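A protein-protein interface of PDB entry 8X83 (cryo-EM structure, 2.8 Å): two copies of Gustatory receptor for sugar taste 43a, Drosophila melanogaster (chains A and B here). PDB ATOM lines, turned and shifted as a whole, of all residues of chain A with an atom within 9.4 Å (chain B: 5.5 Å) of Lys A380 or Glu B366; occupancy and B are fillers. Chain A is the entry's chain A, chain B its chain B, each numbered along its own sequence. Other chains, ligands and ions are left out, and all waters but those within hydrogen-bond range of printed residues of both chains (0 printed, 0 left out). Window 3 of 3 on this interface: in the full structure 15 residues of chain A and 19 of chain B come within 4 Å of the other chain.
Among the printed residues, merely in contact across the chains: Asp A276 with Arg B367, Gln A383 with Glu B366, Gln A383 with Trp B382, Val A387 with Cys B363 and Val A387 with Trp B382.
The indole nitrogen (NE1) of Trp B382 lies within hydrogen-bond range of the side-chain sulfur (SG) of Cys B363 (3.3 Å).
The backbone carbonyl oxygen of Ala A275 is in hydrogen-bond range of the side-chain amide nitrogen of Gln A384, at 3.0 Å.
The backbone carbonyl oxygen (O) of Glu B366 is in hydrogen-bond range of the side-chain amino group (NZ) of Lys A380 (3.4 Å).
OE1 of Gln A384 sits at hydrogen-bond distance from NH1 of Arg B367 (3.3 Å).
NE2 of Gln A383 sits close to NZ of Lys B379 (3.3 Å).
Of chain B, only Glu B366 comes within 4 Å of Lys A380.
Glu B366 touches just these residues of chain A: Lys A380 (3.4 Å) and Gln A383 (3.7 Å).
Cys B363 touches just one residue of chain A: Val A387 (3.8 Å).
Of the printed residues of chain A, Trp B382 touches Gln A383 and Val A387.
Printed residues of chain B within 4 Å of Asp A276: Arg B367 (3.9 Å).
The nearest printed residue of chain B that does not touch Gln A383 is Cys B363 (4.6 Å).
Positions printed for both chains: 362, 366, 378, 379 and 382.
Of the 8 pairs that touch across the chains among the printed residues, none has its exchanged pair printed and touching as well.
Of the 24 printed residues of chain A, 5 touch a printed residue of chain B.
Hydrophobic or aromatic side chains of chain A that line the printed part of chain B: Val A387.
Hydrophobic or aromatic side chains of chain B within 4 Å of the printed part of chain A: Trp B382.
Among the printed residues, 8 pairs touch across the chains.
Among the printed residues, no Asp or Glu carboxylate lies within 4 Å of a Lys or Arg side-chain nitrogen of the other chain.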
ATOM      1  N   GLY A 268     -29.992  22.094 -13.893  1.00  0.00           N
ATOM      2  CA  GLY A 268     -29.506  20.957 -13.133  1.00  0.00           C
ATOM      3  C   GLY A 268     -28.321  20.277 -13.783  1.00  0.00           C
ATOM      4  O   GLY A 268     -27.417  19.800 -13.091  1.00  0.00           O
ATOM      5  N   LEU A 271     -25.447  22.382 -12.816  1.00  0.00           N
ATOM      6  CA  LEU A 271     -25.056  22.106 -11.436  1.00  0.00           C
ATOM      7  C   LEU A 271     -24.296  20.791 -11.322  1.00  0.00           C
ATOM      8  O   LEU A 271     -23.334  20.694 -10.552  1.00  0.00           O
ATOM      9  CB  LEU A 271     -26.285  22.077 -10.531  1.00  0.00           C
ATOM     10  CG  LEU A 271     -25.970  22.080  -9.036  1.00  0.00           C
ATOM     11  CD1 LEU A 271     -25.627  23.478  -8.557  1.00  0.00           C
ATOM     12  CD2 LEU A 271     -27.133  21.516  -8.252  1.00  0.00           C
ATOM     13  N   LYS A 272     -24.719  19.766 -12.063  1.00  0.00           N
ATOM     14  CA  LYS A 272     -23.988  18.504 -12.061  1.00  0.00           C
ATOM     15  C   LYS A 272     -22.575  18.696 -12.592  1.00  0.00           C
ATOM     16  O   LYS A 272     -21.614  18.142 -12.041  1.00  0.00           O
ATOM     17  CB  LYS A 272     -24.735  17.466 -12.896  1.00  0.00           C
ATOM     18  CG  LYS A 272     -24.206  16.050 -12.747  1.00  0.00           C
ATOM     19  CD  LYS A 272     -24.747  15.387 -11.494  1.00  0.00           C
ATOM     20  CE  LYS A 272     -26.138  14.820 -11.725  1.00  0.00           C
ATOM     21  NZ  LYS A 272     -26.897  14.671 -10.455  1.00  0.00           N
ATOM     22  N   ALA A 275     -20.533  20.338  -9.873  1.00  0.00           N
ATOM     23  CA  ALA A 275     -20.153  19.380  -8.839  1.00  0.00           C
ATOM     24  C   ALA A 275     -19.018  18.483  -9.316  1.00  0.00           C
ATOM     25  O   ALA A 275     -18.075  18.200  -8.563  1.00  0.00           O
ATOM     26  CB  ALA A 275     -21.363  18.544  -8.429  1.00  0.00           C
ATOM     27  N   ASP A 276     -19.097  18.021 -10.565  1.00  0.00           N
ATOM     28  CA  ASP A 276     -18.014  17.221 -11.123  1.00  0.00           C
ATOM     29  C   ASP A 276     -16.716  18.016 -11.162  1.00  0.00           C
ATOM     30  O   ASP A 276     -15.644  17.477 -10.872  1.00  0.00           O
ATOM     31  CB  ASP A 276     -18.392  16.735 -12.521  1.00  0.00           C
ATOM     32  CG  ASP A 276     -17.470  15.642 -13.032  1.00  0.00           C
ATOM     33  OD1 ASP A 276     -16.323  15.547 -12.547  1.00  0.00           O
ATOM     34  OD2 ASP A 276     -17.895  14.877 -13.922  1.00  0.00           O
ATOM     35  N   ILE A 359     -19.869  24.977   0.194  1.00  0.00           N
ATOM     36  CA  ILE A 359     -20.973  24.319   0.882  1.00  0.00           C
ATOM     37  C   ILE A 359     -21.984  25.343   1.378  1.00  0.00           C
ATOM     38  O   ILE A 359     -23.188  25.071   1.406  1.00  0.00           O
ATOM     39  CB  ILE A 359     -20.440  23.441   2.028  1.00  0.00           C
ATOM     40  CG1 ILE A 359     -21.522  22.466   2.492  1.00  0.00           C
ATOM     41  CG2 ILE A 359     -19.966  24.301   3.185  1.00  0.00           C
ATOM     42  CD1 ILE A 359     -21.005  21.357   3.374  1.00  0.00           C
ATOM     43  N   VAL A 362     -24.056  26.224  -1.574  1.00  0.00           N
ATOM     44  CA  VAL A 362     -24.985  25.135  -1.853  1.00  0.00           C
ATOM     45  C   VAL A 362     -26.137  25.129  -0.854  1.00  0.00           C
ATOM     46  O   VAL A 362     -27.279  24.836  -1.223  1.00  0.00           O
ATOM     47  CB  VAL A 362     -24.234  23.794  -1.856  1.00  0.00           C
ATOM     48  CG1 VAL A 362     -25.208  22.635  -1.759  1.00  0.00           C
ATOM     49  CG2 VAL A 362     -23.385  23.677  -3.106  1.00  0.00           C
ATOM     50  N   GLU A 366     -30.075  25.368  -1.703  1.00  0.00           N
ATOM     51  CA  GLU A 366     -31.068  24.504  -1.074  1.00  0.00           C
ATOM     52  C   GLU A 366     -32.216  25.329  -0.510  1.00  0.00           C
ATOM     53  O   GLU A 366     -33.394  25.043  -0.751  1.00  0.00           O
ATOM     54  CB  GLU A 366     -30.421  23.680   0.041  1.00  0.00           C
ATOM     55  CG  GLU A 366     -29.558  22.535  -0.431  1.00  0.00           C
ATOM     56  CD  GLU A 366     -29.077  21.663   0.709  1.00  0.00           C
ATOM     57  OE1 GLU A 366     -29.289  22.044   1.880  1.00  0.00           O
ATOM     58  OE2 GLU A 366     -28.485  20.597   0.437  1.00  0.00           O
ATOM     59  N   PRO A 372     -37.916  19.942  -8.227  1.00  0.00           N
ATOM     60  CA  PRO A 372     -37.599  18.611  -7.691  1.00  0.00           C
ATOM     61  C   PRO A 372     -36.230  18.097  -8.113  1.00  0.00           C
ATOM     62  O   PRO A 372     -35.400  17.758  -7.263  1.00  0.00           O
ATOM     63  CB  PRO A 372     -38.722  17.732  -8.257  1.00  0.00           C
ATOM     64  CG  PRO A 372     -39.166  18.436  -9.490  1.00  0.00           C
ATOM     65  CD  PRO A 372     -39.028  19.898  -9.192  1.00  0.00           C
ATOM     66  N   ILE A 373     -35.987  18.031  -9.423  1.00  0.00           N
ATOM     67  CA  ILE A 373     -34.725  17.482  -9.913  1.00  0.00           C
ATOM     68  C   ILE A 373     -33.559  18.375  -9.507  1.00  0.00           C
ATOM     69  O   ILE A 373     -32.498  17.886  -9.099  1.00  0.00           O
ATOM     70  CB  ILE A 373     -34.788  17.277 -11.438  1.00  0.00           C
ATOM     71  CG1 ILE A 373     -35.060  18.601 -12.160  1.00  0.00           C
ATOM     72  CG2 ILE A 373     -35.856  16.251 -11.787  1.00  0.00           C
ATOM     73  CD1 ILE A 373     -35.064  18.484 -13.671  1.00  0.00           C
ATOM     74  N   LEU A 374     -33.733  19.693  -9.607  1.00  0.00           N
ATOM     75  CA  LEU A 374     -32.667  20.604  -9.207  1.00  0.00           C
ATOM     76  C   LEU A 374     -32.416  20.531  -7.708  1.00  0.00           C
ATOM     77  O   LEU A 374     -31.265  20.578  -7.261  1.00  0.00           O
ATOM     78  CB  LEU A 374     -33.011  22.030  -9.632  1.00  0.00           C
ATOM     79  CG  LEU A 374     -31.860  23.036  -9.570  1.00  0.00           C
ATOM     80  CD1 LEU A 374     -30.796  22.702 -10.597  1.00  0.00           C
ATOM     81  CD2 LEU A 374     -32.382  24.444  -9.794  1.00  0.00           C
ATOM     82  N   ALA A 375     -33.481  20.413  -6.912  1.00  0.00           N
ATOM     83  CA  ALA A 375     -33.303  20.261  -5.472  1.00  0.00           C
ATOM     84  C   ALA A 375     -32.552  18.978  -5.145  1.00  0.00           C
ATOM     85  O   ALA A 375     -31.685  18.963  -4.265  1.00  0.00           O
ATOM     86  CB  ALA A 375     -34.659  20.284  -4.769  1.00  0.00           C
ATOM     87  N   GLU A 376     -32.870  17.887  -5.846  1.00  0.00           N
ATOM     88  CA  GLU A 376     -32.151  16.637  -5.625  1.00  0.00           C
ATOM     89  C   GLU A 376     -30.684  16.762  -6.019  1.00  0.00           C
ATOM     90  O   GLU A 376     -29.807  16.237  -5.323  1.00  0.00           O
ATOM     91  CB  GLU A 376     -32.817  15.506  -6.408  1.00  0.00           C
ATOM     92  CG  GLU A 376     -32.195  14.137  -6.177  1.00  0.00           C
ATOM     93  CD  GLU A 376     -32.468  13.604  -4.784  1.00  0.00           C
ATOM     94  OE1 GLU A 376     -31.768  14.024  -3.839  1.00  0.00           O
ATOM     95  OE2 GLU A 376     -33.382  12.766  -4.634  1.00  0.00           O
ATOM     96  N   ALA A 377     -30.399  17.446  -7.129  1.00  0.00           N
ATOM     97  CA  ALA A 377     -29.012  17.652  -7.535  1.00  0.00           C
ATOM     98  C   ALA A 377     -28.260  18.477  -6.497  1.00  0.00           C
ATOM     99  O   ALA A 377     -27.098  18.193  -6.180  1.00  0.00           O
ATOM    100  CB  ALA A 377     -28.963  18.331  -8.903  1.00  0.00           C
ATOM    101  N   VAL A 378     -28.912  19.505  -5.953  1.00  0.00           N
ATOM    102  CA  VAL A 378     -28.272  20.335  -4.936  1.00  0.00           C
ATOM    103  C   VAL A 378     -28.036  19.529  -3.666  1.00  0.00           C
ATOM    104  O   VAL A 378     -27.022  19.704  -2.981  1.00  0.00           O
ATOM    105  CB  VAL A 378     -29.119  21.594  -4.667  1.00  0.00           C
ATOM    106  CG1 VAL A 378     -28.536  22.395  -3.525  1.00  0.00           C
ATOM    107  CG2 VAL A 378     -29.206  22.456  -5.916  1.00  0.00           C
ATOM    108  N   LYS A 379     -28.973  18.644  -3.321  1.00  0.00           N
ATOM    109  CA  LYS A 379     -28.776  17.762  -2.175  1.00  0.00           C
ATOM    110  C   LYS A 379     -27.581  16.844  -2.397  1.00  0.00           C
ATOM    111  O   LYS A 379     -26.763  16.638  -1.492  1.00  0.00           O
ATOM    112  CB  LYS A 379     -30.049  16.948  -1.931  1.00  0.00           C
ATOM    113  CG  LYS A 379     -30.064  16.059  -0.684  1.00  0.00           C
ATOM    114  CD  LYS A 379     -29.237  16.598   0.472  1.00  0.00           C
ATOM    115  CE  LYS A 379     -29.289  15.655   1.664  1.00  0.00           C
ATOM    116  NZ  LYS A 379     -30.463  15.917   2.539  1.00  0.00           N
ATOM    117  N   LYS A 380     -27.465  16.284  -3.601  1.00  0.00           N
ATOM    118  CA  LYS A 380     -26.316  15.447  -3.923  1.00  0.00           C
ATOM    119  C   LYS A 380     -25.020  16.239  -3.795  1.00  0.00           C
ATOM    120  O   LYS A 380     -24.016  15.736  -3.278  1.00  0.00           O
ATOM    121  CB  LYS A 380     -26.467  14.889  -5.340  1.00  0.00           C
ATOM    122  CG  LYS A 380     -27.278  13.598  -5.462  1.00  0.00           C
ATOM    123  CD  LYS A 380     -26.975  12.585  -4.360  1.00  0.00           C
ATOM    124  CE  LYS A 380     -27.416  11.167  -4.719  1.00  0.00           C
ATOM    125  NZ  LYS A 380     -27.306  10.832  -6.170  1.00  0.00           N
ATOM    126  N   PHE A 381     -25.028  17.487  -4.265  1.00  0.00           N
ATOM    127  CA  PHE A 381     -23.834  18.321  -4.181  1.00  0.00           C
ATOM    128  C   PHE A 381     -23.472  18.630  -2.731  1.00  0.00           C
ATOM    129  O   PHE A 381     -22.293  18.612  -2.359  1.00  0.00           O
ATOM    130  CB  PHE A 381     -24.055  19.610  -4.976  1.00  0.00           C
ATOM    131  CG  PHE A 381     -22.792  20.364  -5.306  1.00  0.00           C
ATOM    132  CD1 PHE A 381     -21.543  19.873  -4.963  1.00  0.00           C
ATOM    133  CD2 PHE A 381     -22.864  21.568  -5.983  1.00  0.00           C
ATOM    134  CE1 PHE A 381     -20.399  20.575  -5.278  1.00  0.00           C
ATOM    135  CE2 PHE A 381     -21.722  22.270  -6.300  1.00  0.00           C
ATOM    136  CZ  PHE A 381     -20.488  21.774  -5.947  1.00  0.00           C
ATOM    137  N   TRP A 382     -24.473  18.925  -1.899  1.00  0.00           N
ATOM    138  CA  TRP A 382     -24.218  19.174  -0.483  1.00  0.00           C
ATOM    139  C   TRP A 382     -23.629  17.941   0.187  1.00  0.00           C
ATOM    140  O   TRP A 382     -22.686  18.038   0.982  1.00  0.00           O
ATOM    141  CB  TRP A 382     -25.512  19.595   0.212  1.00  0.00           C
ATOM    142  CG  TRP A 382     -25.329  19.985   1.645  1.00  0.00           C
ATOM    143  CD1 TRP A 382     -24.966  21.210   2.120  1.00  0.00           C
ATOM    144  CD2 TRP A 382     -25.500  19.146   2.793  1.00  0.00           C
ATOM    145  NE1 TRP A 382     -24.898  21.186   3.491  1.00  0.00           N
ATOM    146  CE2 TRP A 382     -25.222  19.929   3.928  1.00  0.00           C
ATOM    147  CE3 TRP A 382     -25.860  17.807   2.969  1.00  0.00           C
ATOM    148  CZ2 TRP A 382     -25.293  19.419   5.222  1.00  0.00           C
ATOM    149  CZ3 TRP A 382     -25.930  17.303   4.254  1.00  0.00           C
ATOM    150  CH2 TRP A 382     -25.648  18.107   5.363  1.00  0.00           C
ATOM    151  N   GLN A 383     -24.186  16.768  -0.116  1.00  0.00           N
ATOM    152  CA  GLN A 383     -23.637  15.525   0.412  1.00  0.00           C
ATOM    153  C   GLN A 383     -22.196  15.321  -0.032  1.00  0.00           C
ATOM    154  O   GLN A 383     -21.351  14.897   0.765  1.00  0.00           O
ATOM    155  CB  GLN A 383     -24.499  14.351  -0.041  1.00  0.00           C
ATOM    156  CG  GLN A 383     -24.778  13.313   1.028  1.00  0.00           C
ATOM    157  CD  GLN A 383     -26.170  12.731   0.909  1.00  0.00           C
ATOM    158  OE1 GLN A 383     -27.156  13.463   0.823  1.00  0.00           O
ATOM    159  NE2 GLN A 383     -26.254  11.408   0.876  1.00  0.00           N
ATOM    160  N   GLN A 384     -21.901  15.611  -1.300  1.00  0.00           N
ATOM    161  CA  GLN A 384     -20.537  15.480  -1.800  1.00  0.00           C
ATOM    162  C   GLN A 384     -19.590  16.416  -1.062  1.00  0.00           C
ATOM    163  O   GLN A 384     -18.478  16.021  -0.691  1.00  0.00           O
ATOM    164  CB  GLN A 384     -20.520  15.759  -3.304  1.00  0.00           C
ATOM    165  CG  GLN A 384     -19.146  15.887  -3.935  1.00  0.00           C
ATOM    166  CD  GLN A 384     -19.224  16.324  -5.383  1.00  0.00           C
ATOM    167  OE1 GLN A 384     -20.015  15.793  -6.162  1.00  0.00           O
ATOM    168  NE2 GLN A 384     -18.415  17.310  -5.748  1.00  0.00           N
ATOM    169  N   LEU A 385     -20.015  17.659  -0.835  1.00  0.00           N
ATOM    170  CA  LEU A 385     -19.167  18.646  -0.178  1.00  0.00           C
ATOM    171  C   LEU A 385     -18.986  18.377   1.309  1.00  0.00           C
ATOM    172  O   LEU A 385     -17.970  18.789   1.877  1.00  0.00           O
ATOM    173  CB  LEU A 385     -19.752  20.044  -0.367  1.00  0.00           C
ATOM    174  CG  LEU A 385     -19.846  20.535  -1.807  1.00  0.00           C
ATOM    175  CD1 LEU A 385     -20.724  21.761  -1.881  1.00  0.00           C
ATOM    176  CD2 LEU A 385     -18.470  20.831  -2.348  1.00  0.00           C
ATOM    177  N   LEU A 386     -19.946  17.710   1.951  1.00  0.00           N
ATOM    178  CA  LEU A 386     -19.829  17.461   3.384  1.00  0.00           C
ATOM    179  C   LEU A 386     -18.580  16.659   3.725  1.00  0.00           C
ATOM    180  O   LEU A 386     -18.060  16.771   4.841  1.00  0.00           O
ATOM    181  CB  LEU A 386     -21.072  16.731   3.890  1.00  0.00           C
ATOM    182  CG  LEU A 386     -21.333  16.803   5.397  1.00  0.00           C
ATOM    183  CD1 LEU A 386     -21.600  18.232   5.841  1.00  0.00           C
ATOM    184  CD2 LEU A 386     -22.490  15.897   5.774  1.00  0.00           C
ATOM    185  N   VAL A 387     -18.081  15.855   2.787  1.00  0.00           N
ATOM    186  CA  VAL A 387     -16.979  14.937   3.065  1.00  0.00           C
ATOM    187  C   VAL A 387     -15.784  15.253   2.176  1.00  0.00           C
ATOM    188  O   VAL A 387     -15.007  14.359   1.824  1.00  0.00           O
ATOM    189  CB  VAL A 387     -17.427  13.477   2.876  1.00  0.00           C
ATOM    190  CG1 VAL A 387     -18.695  13.208   3.665  1.00  0.00           C
ATOM    191  CG2 VAL A 387     -17.639  13.168   1.401  1.00  0.00           C
ATOM    192  N   ILE B 361     -15.217   7.008  -2.542  1.00  0.00           N
ATOM    193  CA  ILE B 361     -15.665   5.972  -3.466  1.00  0.00           C
ATOM    194  C   ILE B 361     -17.163   5.747  -3.311  1.00  0.00           C
ATOM    195  O   ILE B 361     -17.892   5.606  -4.300  1.00  0.00           O
ATOM    196  CB  ILE B 361     -14.868   4.673  -3.238  1.00  0.00           C
ATOM    197  CG1 ILE B 361     -13.365   4.948  -3.334  1.00  0.00           C
ATOM    198  CG2 ILE B 361     -15.274   3.615  -4.251  1.00  0.00           C
ATOM    199  CD1 ILE B 361     -12.504   3.738  -3.073  1.00  0.00           C
ATOM    200  N   VAL B 362     -17.645   5.711  -2.069  1.00  0.00           N
ATOM    201  CA  VAL B 362     -19.070   5.509  -1.837  1.00  0.00           C
ATOM    202  C   VAL B 362     -19.885   6.676  -2.382  1.00  0.00           C
ATOM    203  O   VAL B 362     -20.983   6.476  -2.912  1.00  0.00           O
ATOM    204  CB  VAL B 362     -19.331   5.291  -0.339  1.00  0.00           C
ATOM    205  CG1 VAL B 362     -20.805   5.461  -0.021  1.00  0.00           C
ATOM    206  CG2 VAL B 362     -18.850   3.915   0.078  1.00  0.00           C
ATOM    207  N   CYS B 363     -19.379   7.904  -2.256  1.00  0.00           N
ATOM    208  CA  CYS B 363     -20.052   9.045  -2.866  1.00  0.00           C
ATOM    209  C   CYS B 363     -20.113   8.894  -4.379  1.00  0.00           C
ATOM    210  O   CYS B 363     -21.126   9.227  -5.007  1.00  0.00           O
ATOM    211  CB  CYS B 363     -19.335  10.341  -2.489  1.00  0.00           C
ATOM    212  SG  CYS B 363     -19.722  10.957  -0.837  1.00  0.00           S
ATOM    213  N   GLU B 364     -19.032   8.397  -4.983  1.00  0.00           N
ATOM    214  CA  GLU B 364     -19.045   8.146  -6.420  1.00  0.00           C
ATOM    215  C   GLU B 364     -20.118   7.128  -6.791  1.00  0.00           C
ATOM    216  O   GLU B 364     -20.861   7.325  -7.762  1.00  0.00           O
ATOM    217  CB  GLU B 364     -17.669   7.667  -6.877  1.00  0.00           C
ATOM    218  CG  GLU B 364     -16.647   8.783  -7.021  1.00  0.00           C
ATOM    219  CD  GLU B 364     -15.273   8.271  -7.401  1.00  0.00           C
ATOM    220  OE1 GLU B 364     -15.168   7.527  -8.399  1.00  0.00           O
ATOM    221  OE2 GLU B 364     -14.296   8.613  -6.702  1.00  0.00           O
ATOM    222  N   ILE B 365     -20.222   6.039  -6.026  1.00  0.00           N
ATOM    223  CA  ILE B 365     -21.271   5.054  -6.294  1.00  0.00           C
ATOM    224  C   ILE B 365     -22.646   5.697  -6.163  1.00  0.00           C
ATOM    225  O   ILE B 365     -23.530   5.482  -7.003  1.00  0.00           O
ATOM    226  CB  ILE B 365     -21.136   3.825  -5.373  1.00  0.00           C
ATOM    227  CG1 ILE B 365     -19.694   3.313  -5.338  1.00  0.00           C
ATOM    228  CG2 ILE B 365     -22.074   2.715  -5.828  1.00  0.00           C
ATOM    229  CD1 ILE B 365     -19.501   2.070  -4.498  1.00  0.00           C
ATOM    230  N   GLU B 366     -22.853   6.491  -5.111  1.00  0.00           N
ATOM    231  CA  GLU B 366     -24.113   7.208  -4.951  1.00  0.00           C
ATOM    232  C   GLU B 366     -24.438   8.006  -6.207  1.00  0.00           C
ATOM    233  O   GLU B 366     -25.549   7.938  -6.743  1.00  0.00           O
ATOM    234  CB  GLU B 366     -24.038   8.145  -3.744  1.00  0.00           C
ATOM    235  CG  GLU B 366     -24.128   7.460  -2.401  1.00  0.00           C
ATOM    236  CD  GLU B 366     -24.209   8.444  -1.252  1.00  0.00           C
ATOM    237  OE1 GLU B 366     -24.039   9.657  -1.496  1.00  0.00           O
ATOM    238  OE2 GLU B 366     -24.443   8.006  -0.107  1.00  0.00           O
ATOM    239  N   ARG B 367     -23.461   8.770  -6.687  1.00  0.00           N
ATOM    240  CA  ARG B 367     -23.645   9.636  -7.843  1.00  0.00           C
ATOM    241  C   ARG B 367     -23.860   8.827  -9.116  1.00  0.00           C
ATOM    242  O   ARG B 367     -24.398   9.346 -10.100  1.00  0.00           O
ATOM    243  CB  ARG B 367     -22.435  10.556  -7.993  1.00  0.00           C
ATOM    244  CG  ARG B 367     -22.729  11.893  -8.644  1.00  0.00           C
ATOM    245  CD  ARG B 367     -21.449  12.577  -9.106  1.00  0.00           C
ATOM    246  NE  ARG B 367     -20.334  12.345  -8.193  1.00  0.00           N
ATOM    247  CZ  ARG B 367     -19.253  13.109  -8.121  1.00  0.00           C
ATOM    248  NH1 ARG B 367     -19.094  14.162  -8.905  1.00  0.00           N
ATOM    249  NH2 ARG B 367     -18.305  12.805  -7.239  1.00  0.00           N
ATOM    250  N   LYS B 368     -23.446   7.557  -9.111  1.00  0.00           N
ATOM    251  CA  LYS B 368     -23.545   6.718 -10.300  1.00  0.00           C
ATOM    252  C   LYS B 368     -24.598   5.621 -10.165  1.00  0.00           C
ATOM    253  O   LYS B 368     -25.048   5.085 -11.184  1.00  0.00           O
ATOM    254  CB  LYS B 368     -22.174   6.101 -10.622  1.00  0.00           C
ATOM    255  CG  LYS B 368     -22.207   4.716 -11.256  1.00  0.00           C
ATOM    256  CD  LYS B 368     -20.887   4.400 -11.940  1.00  0.00           C
ATOM    257  CE  LYS B 368     -20.760   2.923 -12.257  1.00  0.00           C
ATOM    258  NZ  LYS B 368     -19.897   2.676 -13.445  1.00  0.00           N
ATOM    259  N   VAL B 369     -25.021   5.286  -8.948  1.00  0.00           N
ATOM    260  CA  VAL B 369     -25.981   4.214  -8.708  1.00  0.00           C
ATOM    261  C   VAL B 369     -27.389   4.765  -8.879  1.00  0.00           C
ATOM    262  O   VAL B 369     -27.649   5.937  -8.579  1.00  0.00           O
ATOM    263  CB  VAL B 369     -25.805   3.598  -7.307  1.00  0.00           C
ATOM    264  CG1 VAL B 369     -26.368   4.527  -6.241  1.00  0.00           C
ATOM    265  CG2 VAL B 369     -26.472   2.234  -7.242  1.00  0.00           C
ATOM    266  N   VAL B 378     -25.978   1.707  -0.514  1.00  0.00           N
ATOM    267  CA  VAL B 378     -24.879   2.663  -0.608  1.00  0.00           C
ATOM    268  C   VAL B 378     -25.100   3.819   0.359  1.00  0.00           C
ATOM    269  O   VAL B 378     -24.149   4.343   0.951  1.00  0.00           O
ATOM    270  CB  VAL B 378     -24.723   3.153  -2.060  1.00  0.00           C
ATOM    271  CG1 VAL B 378     -23.676   4.240  -2.147  1.00  0.00           C
ATOM    272  CG2 VAL B 378     -24.350   1.998  -2.976  1.00  0.00           C
ATOM    273  N   LYS B 379     -26.352   4.246   0.525  1.00  0.00           N
ATOM    274  CA  LYS B 379     -26.660   5.281   1.507  1.00  0.00           C
ATOM    275  C   LYS B 379     -26.330   4.806   2.916  1.00  0.00           C
ATOM    276  O   LYS B 379     -25.752   5.551   3.717  1.00  0.00           O
ATOM    277  CB  LYS B 379     -28.137   5.668   1.397  1.00  0.00           C
ATOM    278  CG  LYS B 379     -28.605   6.836   2.270  1.00  0.00           C
ATOM    279  CD  LYS B 379     -27.532   7.879   2.539  1.00  0.00           C
ATOM    280  CE  LYS B 379     -28.067   8.995   3.423  1.00  0.00           C
ATOM    281  NZ  LYS B 379     -28.741  10.063   2.637  1.00  0.00           N
ATOM    282  N   TRP B 382     -22.577   4.944   3.283  1.00  0.00           N
ATOM    283  CA  TRP B 382     -22.108   6.314   3.466  1.00  0.00           C
ATOM    284  C   TRP B 382     -22.371   6.793   4.887  1.00  0.00           C
ATOM    285  O   TRP B 382     -21.516   7.431   5.513  1.00  0.00           O
ATOM    286  CB  TRP B 382     -22.789   7.236   2.455  1.00  0.00           C
ATOM    287  CG  TRP B 382     -22.285   8.644   2.488  1.00  0.00           C
ATOM    288  CD1 TRP B 382     -21.196   9.140   1.835  1.00  0.00           C
ATOM    289  CD2 TRP B 382     -22.851   9.743   3.213  1.00  0.00           C
ATOM    290  NE1 TRP B 382     -21.048  10.477   2.107  1.00  0.00           N
ATOM    291  CE2 TRP B 382     -22.052  10.871   2.952  1.00  0.00           C
ATOM    292  CE3 TRP B 382     -23.956   9.881   4.057  1.00  0.00           C
ATOM    293  CZ2 TRP B 382     -22.322  12.121   3.504  1.00  0.00           C
ATOM    294  CZ3 TRP B 382     -24.222  11.121   4.605  1.00  0.00           C
ATOM    295  CH2 TRP B 382     -23.409  12.224   4.327  1.00  0.00           C
